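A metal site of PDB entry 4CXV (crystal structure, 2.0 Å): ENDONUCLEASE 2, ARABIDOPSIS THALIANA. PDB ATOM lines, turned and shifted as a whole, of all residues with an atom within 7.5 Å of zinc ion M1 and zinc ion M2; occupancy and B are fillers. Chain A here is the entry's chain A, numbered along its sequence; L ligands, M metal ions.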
ATOM      1  N   TRP A   1     -29.860  -0.177  22.386  1.00  0.00           N
ATOM      2  CA  TRP A   1     -31.245   0.317  22.308  1.00  0.00           C
ATOM      3  C   TRP A   1     -31.305   1.821  22.283  1.00  0.00           C
ATOM      4  O   TRP A   1     -30.425   2.493  22.791  1.00  0.00           O
ATOM      5  CB  TRP A   1     -32.104  -0.138  23.507  1.00  0.00           C
ATOM      6  CG  TRP A   1     -31.976  -1.569  23.834  1.00  0.00           C
ATOM      7  CD1 TRP A   1     -31.212  -2.103  24.808  1.00  0.00           C
ATOM      8  CD2 TRP A   1     -32.686  -2.665  23.224  1.00  0.00           C
ATOM      9  NE1 TRP A   1     -31.371  -3.477  24.829  1.00  0.00           N
ATOM     10  CE2 TRP A   1     -32.262  -3.836  23.853  1.00  0.00           C
ATOM     11  CE3 TRP A   1     -33.632  -2.743  22.188  1.00  0.00           C
ATOM     12  CZ2 TRP A   1     -32.734  -5.095  23.478  1.00  0.00           C
ATOM     13  CZ3 TRP A   1     -34.099  -3.990  21.829  1.00  0.00           C
ATOM     14  CH2 TRP A   1     -33.639  -5.153  22.466  1.00  0.00           C
ATOM     15  N   GLY A   2     -32.395   2.324  21.731  1.00  0.00           N
ATOM     16  CA  GLY A   2     -32.762   3.738  21.906  1.00  0.00           C
ATOM     17  C   GLY A   2     -33.383   3.989  23.271  1.00  0.00           C
ATOM     18  O   GLY A   2     -33.350   3.169  24.173  1.00  0.00           O
ATOM     19  N   LYS A   3     -33.981   5.152  23.391  1.00  0.00           N
ATOM     20  CA  LYS A   3     -34.461   5.642  24.678  1.00  0.00           C
ATOM     21  C   LYS A   3     -35.441   4.702  25.325  1.00  0.00           C
ATOM     22  O   LYS A   3     -35.355   4.409  26.517  1.00  0.00           O
ATOM     23  CB  LYS A   3     -35.185   6.982  24.449  1.00  0.00           C
ATOM     24  CG  LYS A   3     -35.568   7.715  25.735  1.00  0.00           C
ATOM     25  CD  LYS A   3     -36.912   7.296  26.275  1.00  0.00           C
ATOM     26  CE  LYS A   3     -37.823   8.496  26.522  1.00  0.00           C
ATOM     27  NZ  LYS A   3     -37.163   9.580  27.264  1.00  0.00           N
ATOM     28  N   GLY A   5     -36.097   1.451  24.915  1.00  0.00           N
ATOM     29  CA  GLY A   5     -35.563   0.172  25.383  1.00  0.00           C
ATOM     30  C   GLY A   5     -34.820   0.309  26.702  1.00  0.00           C
ATOM     31  O   GLY A   5     -35.004  -0.480  27.599  1.00  0.00           O
ATOM     32  N   HIS A   6     -33.940   1.306  26.793  1.00  0.00           N
ATOM     33  CA  HIS A   6     -33.203   1.513  28.047  1.00  0.00           C
ATOM     34  C   HIS A   6     -34.141   1.873  29.205  1.00  0.00           C
ATOM     35  O   HIS A   6     -33.930   1.428  30.332  1.00  0.00           O
ATOM     36  CB  HIS A   6     -32.085   2.565  27.870  1.00  0.00           C
ATOM     37  CG  HIS A   6     -30.920   2.085  27.060  1.00  0.00           C
ATOM     38  ND1 HIS A   6     -29.988   1.214  27.561  1.00  0.00           N
ATOM     39  CD2 HIS A   6     -30.551   2.342  25.786  1.00  0.00           C
ATOM     40  CE1 HIS A   6     -29.071   0.975  26.642  1.00  0.00           C
ATOM     41  NE2 HIS A   6     -29.418   1.608  25.544  1.00  0.00           N
ATOM     42  N   CYS A  41     -30.751   6.325  32.227  1.00  0.00           N
ATOM     43  CA  CYS A  41     -30.219   5.137  31.529  1.00  0.00           C
ATOM     44  C   CYS A  41     -29.838   5.375  30.080  1.00  0.00           C
ATOM     45  O   CYS A  41     -29.335   4.472  29.430  1.00  0.00           O
ATOM     46  CB  CYS A  41     -31.104   3.919  31.705  1.00  0.00           C
ATOM     47  SG  CYS A  41     -31.000   3.322  33.410  1.00  0.00           S
ATOM     48  N   LEU A  42     -29.985   6.609  29.599  1.00  0.00           N
ATOM     49  CA  LEU A  42     -29.414   7.019  28.308  1.00  0.00           C
ATOM     50  C   LEU A  42     -28.176   7.928  28.456  1.00  0.00           C
ATOM     51  O   LEU A  42     -27.592   8.321  27.463  1.00  0.00           O
ATOM     52  CB  LEU A  42     -30.474   7.690  27.429  1.00  0.00           C
ATOM     53  CG  LEU A  42     -30.506   7.324  25.949  1.00  0.00           C
ATOM     54  CD1 LEU A  42     -30.837   5.840  25.719  1.00  0.00           C
ATOM     55  CD2 LEU A  42     -31.534   8.197  25.282  1.00  0.00           C
ATOM     56  N   ALA A  44     -25.150   7.342  29.117  1.00  0.00           N
ATOM     57  CA  ALA A  44     -23.955   6.878  28.429  1.00  0.00           C
ATOM     58  C   ALA A  44     -23.967   7.247  26.955  1.00  0.00           C
ATOM     59  O   ALA A  44     -22.918   7.466  26.381  1.00  0.00           O
ATOM     60  CB  ALA A  44     -23.743   5.380  28.597  1.00  0.00           C
ATOM     61  N   ASP A  45     -25.129   7.221  26.319  1.00  0.00           N
ATOM     62  CA  ASP A  45     -25.151   7.546  24.883  1.00  0.00           C
ATOM     63  C   ASP A  45     -24.715   9.009  24.620  1.00  0.00           C
ATOM     64  O   ASP A  45     -24.145   9.294  23.586  1.00  0.00           O
ATOM     65  CB  ASP A  45     -26.539   7.308  24.266  1.00  0.00           C
ATOM     66  CG  ASP A  45     -26.720   5.863  23.743  1.00  0.00           C
ATOM     67  OD1 ASP A  45     -25.786   5.032  23.815  1.00  0.00           O
ATOM     68  OD2 ASP A  45     -27.826   5.574  23.271  1.00  0.00           O
ATOM     69  N   LYS A  48     -20.700   9.612  24.288  1.00  0.00           N
ATOM     70  CA  LYS A  48     -19.939   8.949  23.230  1.00  0.00           C
ATOM     71  C   LYS A  48     -18.791   9.779  22.653  1.00  0.00           C
ATOM     72  O   LYS A  48     -17.831   9.193  22.167  1.00  0.00           O
ATOM     73  CB  LYS A  48     -20.875   8.482  22.117  1.00  0.00           C
ATOM     74  CG  LYS A  48     -21.709   7.284  22.486  1.00  0.00           C
ATOM     75  CD  LYS A  48     -22.451   6.741  21.264  1.00  0.00           C
ATOM     76  CE  LYS A  48     -23.327   5.584  21.627  1.00  0.00           C
ATOM     77  NZ  LYS A  48     -24.315   5.267  20.545  1.00  0.00           N
ATOM     78  N   SER A  55     -17.076   5.102  23.273  1.00  0.00           N
ATOM     79  CA  SER A  55     -17.989   4.711  22.185  1.00  0.00           C
ATOM     80  C   SER A  55     -17.913   3.229  21.805  1.00  0.00           C
ATOM     81  O   SER A  55     -18.943   2.627  21.503  1.00  0.00           O
ATOM     82  CB  SER A  55     -18.027   5.596  20.917  1.00  0.00           C
ATOM     83  OG  SER A  55     -16.836   6.269  20.635  1.00  0.00           O
ATOM     84  N   LEU A  57     -17.500   0.878  23.768  1.00  0.00           N
ATOM     85  CA  LEU A  57     -18.006   0.108  24.889  1.00  0.00           C
ATOM     86  C   LEU A  57     -19.488  -0.226  24.775  1.00  0.00           C
ATOM     87  O   LEU A  57     -19.999  -0.943  25.631  1.00  0.00           O
ATOM     88  CB  LEU A  57     -17.754   0.877  26.200  1.00  0.00           C
ATOM     89  CG  LEU A  57     -16.302   1.302  26.476  1.00  0.00           C
ATOM     90  CD1 LEU A  57     -16.176   1.936  27.856  1.00  0.00           C
ATOM     91  CD2 LEU A  57     -15.331   0.128  26.346  1.00  0.00           C
ATOM     92  N   HIS A  58     -20.171   0.286  23.751  1.00  0.00           N
ATOM     93  CA  HIS A  58     -21.603   0.041  23.603  1.00  0.00           C
ATOM     94  C   HIS A  58     -21.922  -1.248  22.845  1.00  0.00           C
ATOM     95  O   HIS A  58     -23.090  -1.667  22.839  1.00  0.00           O
ATOM     96  CB  HIS A  58     -22.279   1.243  22.915  1.00  0.00           C
ATOM     97  CG  HIS A  58     -22.238   2.503  23.735  1.00  0.00           C
ATOM     98  ND1 HIS A  58     -23.373   3.070  24.268  1.00  0.00           N
ATOM     99  CD2 HIS A  58     -21.218   3.298  24.125  1.00  0.00           C
ATOM    100  CE1 HIS A  58     -23.054   4.165  24.942  1.00  0.00           C
ATOM    101  NE2 HIS A  58     -21.751   4.326  24.871  1.00  0.00           N
ATOM    102  N   TYR A  59     -20.947  -1.889  22.226  1.00  0.00           N
ATOM    103  CA  TYR A  59     -21.249  -3.003  21.337  1.00  0.00           C
ATOM    104  C   TYR A  59     -20.062  -3.971  21.263  1.00  0.00           C
ATOM    105  O   TYR A  59     -19.029  -3.776  21.912  1.00  0.00           O
ATOM    106  CB  TYR A  59     -21.585  -2.459  19.936  1.00  0.00           C
ATOM    107  CG  TYR A  59     -20.471  -1.617  19.361  1.00  0.00           C
ATOM    108  CD1 TYR A  59     -19.372  -2.217  18.761  1.00  0.00           C
ATOM    109  CD2 TYR A  59     -20.459  -0.219  19.515  1.00  0.00           C
ATOM    110  CE1 TYR A  59     -18.320  -1.465  18.264  1.00  0.00           C
ATOM    111  CE2 TYR A  59     -19.429   0.550  18.999  1.00  0.00           C
ATOM    112  CZ  TYR A  59     -18.370  -0.084  18.373  1.00  0.00           C
ATOM    113  OH  TYR A  59     -17.338   0.635  17.897  1.00  0.00           O
ATOM    114  N   VAL A  85     -18.645  -3.976  24.922  1.00  0.00           N
ATOM    115  CA  VAL A  85     -19.664  -3.894  25.960  1.00  0.00           C
ATOM    116  C   VAL A  85     -19.495  -4.937  27.073  1.00  0.00           C
ATOM    117  O   VAL A  85     -19.793  -4.657  28.229  1.00  0.00           O
ATOM    118  CB  VAL A  85     -21.080  -3.819  25.355  1.00  0.00           C
ATOM    119  CG1 VAL A  85     -21.473  -5.144  24.689  1.00  0.00           C
ATOM    120  CG2 VAL A  85     -22.104  -3.385  26.392  1.00  0.00           C
ATOM    121  N   HIS A 120     -26.718   1.208  31.491  1.00  0.00           N
ATOM    122  CA  HIS A 120     -26.873   1.329  30.062  1.00  0.00           C
ATOM    123  C   HIS A 120     -26.273   0.126  29.314  1.00  0.00           C
ATOM    124  O   HIS A 120     -26.896  -0.415  28.407  1.00  0.00           O
ATOM    125  CB  HIS A 120     -26.220   2.621  29.587  1.00  0.00           C
ATOM    126  CG  HIS A 120     -26.354   2.838  28.115  1.00  0.00           C
ATOM    127  ND1 HIS A 120     -27.412   3.522  27.568  1.00  0.00           N
ATOM    128  CD2 HIS A 120     -25.567   2.487  27.091  1.00  0.00           C
ATOM    129  CE1 HIS A 120     -27.252   3.591  26.260  1.00  0.00           C
ATOM    130  NE2 HIS A 120     -26.155   2.941  25.937  1.00  0.00           N
ATOM    131  N   PHE A 121     -25.057  -0.259  29.691  1.00  0.00           N
ATOM    132  CA  PHE A 121     -24.368  -1.334  28.983  1.00  0.00           C
ATOM    133  C   PHE A 121     -25.030  -2.699  29.216  1.00  0.00           C
ATOM    134  O   PHE A 121     -25.054  -3.517  28.304  1.00  0.00           O
ATOM    135  CB  PHE A 121     -22.867  -1.328  29.285  1.00  0.00           C
ATOM    136  CG  PHE A 121     -22.128  -0.068  28.820  1.00  0.00           C
ATOM    137  CD1 PHE A 121     -22.456   0.587  27.645  1.00  0.00           C
ATOM    138  CD2 PHE A 121     -21.070   0.434  29.574  1.00  0.00           C
ATOM    139  CE1 PHE A 121     -21.747   1.688  27.210  1.00  0.00           C
ATOM    140  CE2 PHE A 121     -20.368   1.554  29.153  1.00  0.00           C
ATOM    141  CZ  PHE A 121     -20.720   2.194  27.971  1.00  0.00           C
ATOM    142  N   GLY A 123     -28.121  -3.032  29.331  1.00  0.00           N
ATOM    143  CA  GLY A 123     -29.118  -2.952  28.280  1.00  0.00           C
ATOM    144  C   GLY A 123     -28.565  -3.227  26.904  1.00  0.00           C
ATOM    145  O   GLY A 123     -29.076  -4.087  26.173  1.00  0.00           O
ATOM    146  N   ASP A 124     -27.500  -2.522  26.520  1.00  0.00           N
ATOM    147  CA  ASP A 124     -26.974  -2.661  25.177  1.00  0.00           C
ATOM    148  C   ASP A 124     -26.516  -4.090  24.879  1.00  0.00           C
ATOM    149  O   ASP A 124     -26.677  -4.534  23.755  1.00  0.00           O
ATOM    150  CB  ASP A 124     -25.842  -1.719  24.899  1.00  0.00           C
ATOM    151  CG  ASP A 124     -26.305  -0.401  24.404  1.00  0.00           C
ATOM    152  OD1 ASP A 124     -27.531  -0.165  24.254  1.00  0.00           O
ATOM    153  OD2 ASP A 124     -25.446   0.412  24.187  1.00  0.00           O
ATOM    154  N   ILE A 125     -25.933  -4.798  25.840  1.00  0.00           N
ATOM    155  CA  ILE A 125     -25.459  -6.160  25.576  1.00  0.00           C
ATOM    156  C   ILE A 125     -26.610  -7.114  25.263  1.00  0.00           C
ATOM    157  O   ILE A 125     -26.359  -8.187  24.712  1.00  0.00           O
ATOM    158  CB  ILE A 125     -24.536  -6.685  26.714  1.00  0.00           C
ATOM    159  CG1 ILE A 125     -23.654  -7.818  26.199  1.00  0.00           C
ATOM    160  CG2 ILE A 125     -25.289  -7.112  27.961  1.00  0.00           C
ATOM    161  CD1 ILE A 125     -22.473  -8.152  27.087  1.00  0.00           C
ATOM    162  N   GLN A 127     -29.231  -6.051  23.232  1.00  0.00           N
ATOM    163  CA  GLN A 127     -29.756  -5.699  21.915  1.00  0.00           C
ATOM    164  C   GLN A 127     -28.986  -6.625  20.917  1.00  0.00           C
ATOM    165  O   GLN A 127     -27.761  -6.568  20.835  1.00  0.00           O
ATOM    166  CB  GLN A 127     -29.467  -4.222  21.598  1.00  0.00           C
ATOM    167  CG  GLN A 127     -30.473  -3.546  20.671  1.00  0.00           C
ATOM    168  CD  GLN A 127     -30.309  -3.903  19.212  1.00  0.00           C
ATOM    169  OE1 GLN A 127     -30.365  -5.090  18.827  1.00  0.00           O
ATOM    170  NE2 GLN A 127     -30.188  -2.889  18.369  1.00  0.00           N
ATOM    171  N   HIS A 130     -26.227  -5.277  18.817  1.00  0.00           N
ATOM    172  CA  HIS A 130     -25.024  -4.802  19.491  1.00  0.00           C
ATOM    173  C   HIS A 130     -23.982  -5.908  19.693  1.00  0.00           C
ATOM    174  O   HIS A 130     -22.949  -5.634  20.268  1.00  0.00           O
ATOM    175  CB  HIS A 130     -25.398  -4.120  20.829  1.00  0.00           C
ATOM    176  CG  HIS A 130     -25.849  -2.710  20.664  1.00  0.00           C
ATOM    177  ND1 HIS A 130     -25.172  -1.641  21.215  1.00  0.00           N
ATOM    178  CD2 HIS A 130     -26.893  -2.173  19.978  1.00  0.00           C
ATOM    179  CE1 HIS A 130     -25.775  -0.514  20.891  1.00  0.00           C
ATOM    180  NE2 HIS A 130     -26.834  -0.804  20.153  1.00  0.00           N
ATOM    181  N   HIS A 154     -30.150  -1.900  12.115  1.00  0.00           N
ATOM    182  CA  HIS A 154     -29.739  -1.626  13.475  1.00  0.00           C
ATOM    183  C   HIS A 154     -30.752  -0.749  14.210  1.00  0.00           C
ATOM    184  O   HIS A 154     -31.158  -1.040  15.339  1.00  0.00           O
ATOM    185  CB  HIS A 154     -28.396  -0.977  13.504  1.00  0.00           C
ATOM    186  CG  HIS A 154     -27.836  -0.874  14.872  1.00  0.00           C
ATOM    187  ND1 HIS A 154     -26.997  -1.823  15.412  1.00  0.00           N
ATOM    188  CD2 HIS A 154     -28.078   0.029  15.858  1.00  0.00           C
ATOM    189  CE1 HIS A 154     -26.697  -1.476  16.646  1.00  0.00           C
ATOM    190  NE2 HIS A 154     -27.344  -0.360  16.938  1.00  0.00           N
ATOM    191  N   ASP A 158     -32.894  -1.111  17.593  1.00  0.00           N
ATOM    192  CA  ASP A 158     -32.763  -0.178  18.708  1.00  0.00           C
ATOM    193  C   ASP A 158     -34.104   0.445  19.094  1.00  0.00           C
ATOM    194  O   ASP A 158     -34.400   0.557  20.303  1.00  0.00           O
ATOM    195  CB  ASP A 158     -31.820   0.971  18.368  1.00  0.00           C
ATOM    196  CG  ASP A 158     -30.387   0.665  18.663  1.00  0.00           C
ATOM    197  OD1 ASP A 158     -30.069  -0.316  19.362  1.00  0.00           O
ATOM    198  OD2 ASP A 158     -29.531   1.445  18.183  1.00  0.00           O
HETATM  199  P1  LIG L   1     -27.072   2.805  21.670  1.00  0.00           P
HETATM  200  O1  LIG L   1     -27.648   4.183  21.362  1.00  0.00           O
HETATM  201  O2  LIG L   1     -27.505   2.335  23.029  1.00  0.00           O
HETATM  202  O3  LIG L   1     -25.584   2.767  21.853  1.00  0.00           O
HETATM  203  O4  LIG L   1     -27.715   1.963  20.625  1.00  0.00           O
HETATM  204 ZN    ZN M   1     -25.542   2.568  23.921  1.00  0.00          ZN
HETATM  205 ZN    ZN M   2     -28.829   1.302  23.666  1.00  0.00          ZN
HETATM  206 ZN    ZN M   3     -27.703   0.714  18.909  1.00  0.00          ZN
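A ring nitrogen (ND1) of His 120 lies within hydrogen-bond range of the backbone carbonyl oxygen of Cys 41, 2.8 Å away.
The side-chain carboxylate (OD1) of Asp 45 lies close to the side-chain amino group (NZ) of Lys 48.
ND1 of His 6 sits close to ND1 of His 120.
The backbone carbonyl oxygen of Gly 123 is in hydrogen-bond range of the indole nitrogen of Trp 1 (2.7 Å).
N of Trp 1 sits close to OD1 of Asp 158 (3.0 Å).
A ring nitrogen (ND1) of His 130 is in hydrogen-bond range of the backbone carbonyl oxygen of His 58, 2.6 Å away.
The nearest printed residue that does not touch zinc ion M1 is His 6 (4.3 Å).
Of the 24 residues printed, 4 come within 4 Å of zinc ion M2.
Zinc ion M1 is bound by an oxygen (O3) of the ligand (2.1 Å), a ring nitrogen (NE2) of His 120 (2.1 Å), an oxygen (O2) of the ligand (2.2 Å), the side-chain carboxylate (OD2) of Asp 124 (2.2 Å), a ring nitrogen (ND1) of His 58 (2.3 Å) and the side-chain carboxylate (OD1) of Asp 45 (2.5 Å).
Zinc ion M1 has six donor atoms within binding distance.
Zinc ion M2 is bound by an oxygen (O2) of the ligand (1.8 Å).
Zinc ion M2 is bound by a ring nitrogen (NE2) of His 6 (2.0 Å).
OD1 of Asp 124 binds zinc ion M2 (2.0 Å).
O of Trp 1 binds zinc ion M2 (2.2 Å).
The backbone nitrogen (N) of Trp 1 is bound to zinc ion M2, at 2.2 Å.
Zinc ion M2 has five donor atoms within binding distance.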
